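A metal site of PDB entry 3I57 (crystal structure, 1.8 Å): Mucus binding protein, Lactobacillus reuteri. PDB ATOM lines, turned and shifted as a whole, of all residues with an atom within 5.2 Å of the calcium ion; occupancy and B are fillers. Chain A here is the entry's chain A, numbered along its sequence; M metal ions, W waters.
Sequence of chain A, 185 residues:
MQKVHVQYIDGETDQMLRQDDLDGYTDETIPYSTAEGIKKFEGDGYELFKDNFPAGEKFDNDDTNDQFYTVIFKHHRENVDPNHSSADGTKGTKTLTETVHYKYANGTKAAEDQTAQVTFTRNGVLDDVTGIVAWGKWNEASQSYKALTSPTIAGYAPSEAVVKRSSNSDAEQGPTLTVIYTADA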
ATOM      1  N   GLN A   2     -29.705  16.285 -24.989  1.00  0.00           N
ATOM      2  CA  GLN A   2     -28.808  16.294 -26.156  1.00  0.00           C
ATOM      3  C   GLN A   2     -29.048  15.011 -26.951  1.00  0.00           C
ATOM      4  O   GLN A   2     -29.507  14.016 -26.392  1.00  0.00           O
ATOM      5  CB  GLN A   2     -27.366  16.342 -25.698  1.00  0.00           C
ATOM      6  CG  GLN A   2     -27.037  17.561 -24.818  1.00  0.00           C
ATOM      7  CD  GLN A   2     -27.394  18.851 -25.520  1.00  0.00           C
ATOM      8  OE1 GLN A   2     -27.429  18.905 -26.763  1.00  0.00           O
ATOM      9  NE2 GLN A   2     -27.660  19.912 -24.739  1.00  0.00           N
ATOM     10  N   LYS A   3     -28.692  15.015 -28.229  1.00  0.00           N
ATOM     11  CA  LYS A   3     -28.930  13.849 -29.076  1.00  0.00           C
ATOM     12  C   LYS A   3     -27.667  13.445 -29.770  1.00  0.00           C
ATOM     13  O   LYS A   3     -26.869  14.289 -30.183  1.00  0.00           O
ATOM     14  CB  LYS A   3     -30.002  14.120 -30.148  1.00  0.00           C
ATOM     15  CG  LYS A   3     -31.392  14.349 -29.615  1.00  0.00           C
ATOM     16  CD  LYS A   3     -32.355  14.697 -30.775  1.00  0.00           C
ATOM     17  CE  LYS A   3     -33.759  14.161 -30.509  1.00  0.00           C
ATOM     18  NZ  LYS A   3     -33.792  12.670 -30.243  1.00  0.00           N
ATOM     19  N   ASP A  60     -22.669  16.765 -25.531  1.00  0.00           N
ATOM     20  CA  ASP A  60     -22.200  18.174 -25.548  1.00  0.00           C
ATOM     21  C   ASP A  60     -23.118  19.148 -24.801  1.00  0.00           C
ATOM     22  O   ASP A  60     -24.075  18.751 -24.161  1.00  0.00           O
ATOM     23  CB  ASP A  60     -21.996  18.684 -26.974  1.00  0.00           C
ATOM     24  CG  ASP A  60     -23.280  18.737 -27.785  1.00  0.00           C
ATOM     25  OD1 ASP A  60     -24.407  18.915 -27.255  1.00  0.00           O
ATOM     26  OD2 ASP A  60     -23.146  18.615 -29.014  1.00  0.00           O
ATOM     27  N   ASP A  62     -24.511  21.822 -26.489  1.00  0.00           N
ATOM     28  CA  ASP A  62     -24.909  22.580 -27.678  1.00  0.00           C
ATOM     29  C   ASP A  62     -26.275  22.098 -28.147  1.00  0.00           C
ATOM     30  O   ASP A  62     -26.390  21.047 -28.791  1.00  0.00           O
ATOM     31  CB  ASP A  62     -23.849  22.395 -28.784  1.00  0.00           C
ATOM     32  CG  ASP A  62     -24.182  23.152 -30.054  1.00  0.00           C
ATOM     33  OD1 ASP A  62     -25.344  23.600 -30.181  1.00  0.00           O
ATOM     34  OD2 ASP A  62     -23.295  23.272 -30.922  1.00  0.00           O
ATOM     35  N   ASP A  63     -27.306  22.858 -27.770  1.00  0.00           N
ATOM     36  CA  ASP A  63     -28.699  22.496 -28.020  1.00  0.00           C
ATOM     37  C   ASP A  63     -29.031  22.473 -29.488  1.00  0.00           C
ATOM     38  O   ASP A  63     -29.872  21.702 -29.924  1.00  0.00           O
ATOM     39  CB  ASP A  63     -29.639  23.525 -27.390  1.00  0.00           C
ATOM     40  CG  ASP A  63     -29.712  23.410 -25.902  1.00  0.00           C
ATOM     41  OD1 ASP A  63     -29.022  22.533 -25.355  1.00  0.00           O
ATOM     42  OD2 ASP A  63     -30.435  24.240 -25.282  1.00  0.00           O
ATOM     43  N   ASN A  65     -27.141  21.814 -32.185  1.00  0.00           N
ATOM     44  CA  ASN A  65     -26.521  20.800 -33.026  1.00  0.00           C
ATOM     45  C   ASN A  65     -26.433  19.428 -32.340  1.00  0.00           C
ATOM     46  O   ASN A  65     -26.051  19.345 -31.152  1.00  0.00           O
ATOM     47  CB  ASN A  65     -25.122  21.267 -33.392  1.00  0.00           C
ATOM     48  CG  ASN A  65     -25.134  22.593 -34.156  1.00  0.00           C
ATOM     49  OD1 ASN A  65     -24.561  23.591 -33.705  1.00  0.00           O
ATOM     50  ND2 ASN A  65     -25.811  22.605 -35.299  1.00  0.00           N
ATOM     51  N   ASP A  66     -26.777  18.380 -33.078  1.00  0.00           N
ATOM     52  CA  ASP A  66     -26.586  17.002 -32.598  1.00  0.00           C
ATOM     53  C   ASP A  66     -25.164  16.503 -32.870  1.00  0.00           C
ATOM     54  O   ASP A  66     -24.419  17.090 -33.676  1.00  0.00           O
ATOM     55  CB  ASP A  66     -27.591  16.046 -33.281  1.00  0.00           C
ATOM     56  CG  ASP A  66     -29.038  16.337 -32.913  1.00  0.00           C
ATOM     57  OD1 ASP A  66     -29.272  17.131 -31.989  1.00  0.00           O
ATOM     58  OD2 ASP A  66     -29.943  15.770 -33.544  1.00  0.00           O
ATOM     59  N   GLN A  67     -24.809  15.402 -32.215  1.00  0.00           N
ATOM     60  CA  GLN A  67     -23.506  14.776 -32.406  1.00  0.00           C
ATOM     61  C   GLN A  67     -23.689  13.585 -33.332  1.00  0.00           C
ATOM     62  O   GLN A  67     -24.586  12.793 -33.116  1.00  0.00           O
ATOM     63  CB  GLN A  67     -22.946  14.321 -31.055  1.00  0.00           C
ATOM     64  CG  GLN A  67     -22.475  15.500 -30.182  1.00  0.00           C
ATOM     65  CD  GLN A  67     -22.330  15.119 -28.719  1.00  0.00           C
ATOM     66  OE1 GLN A  67     -21.301  14.550 -28.304  1.00  0.00           O
ATOM     67  NE2 GLN A  67     -23.322  15.449 -27.940  1.00  0.00           N
HETATM   68 CA    CA M   1     -26.163  18.809 -28.864  1.00  0.00          CA
HETATM   69  O   HOH W   1     -25.651  16.495 -28.930  1.00  0.00           O
HETATM   70  O   HOH W   2     -28.409  17.895 -29.476  1.00  0.00           O
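The side-chain amide oxygen (OD1) of Asn 65 sits close to the side-chain carboxylate (OD2) of Asp 62, at 3.1 Å. The side-chain amide nitrogen (NE2) of Gln 67 sits close to the backbone NH (N) of Asp 60, 2.8 Å away. OD1 of Asp 63 lies within hydrogen-bond range of NE2 of Gln 2.
Of the 8 residues printed, 4 come within 4 Å of the calcium ion. The nearest printed residue that does not touch the calcium ion is Asp 66 (4.2 Å).
The calcium ion is bound by the backbone carbonyl oxygen of Asp 62, the backbone carbonyl oxygen of Asn 65, water W1, the side-chain carboxylate of Asp 60, the side-chain amide oxygen of Gln 2 and water W2. Slightly farther from the calcium ion lies OD2 of Asp 60 (3.0 Å).
Water W2 lies within hydrogen-bond range of the side-chain carboxylate of Asp 66 (2.8 Å) and the backbone NH of Lys 3 (3.2 Å). Water W1 lies within hydrogen-bond range of NE2 of Gln 67 (2.7 Å), O of Lys 3 (2.8 Å) and OD2 of Asp 60 (3.3 Å).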
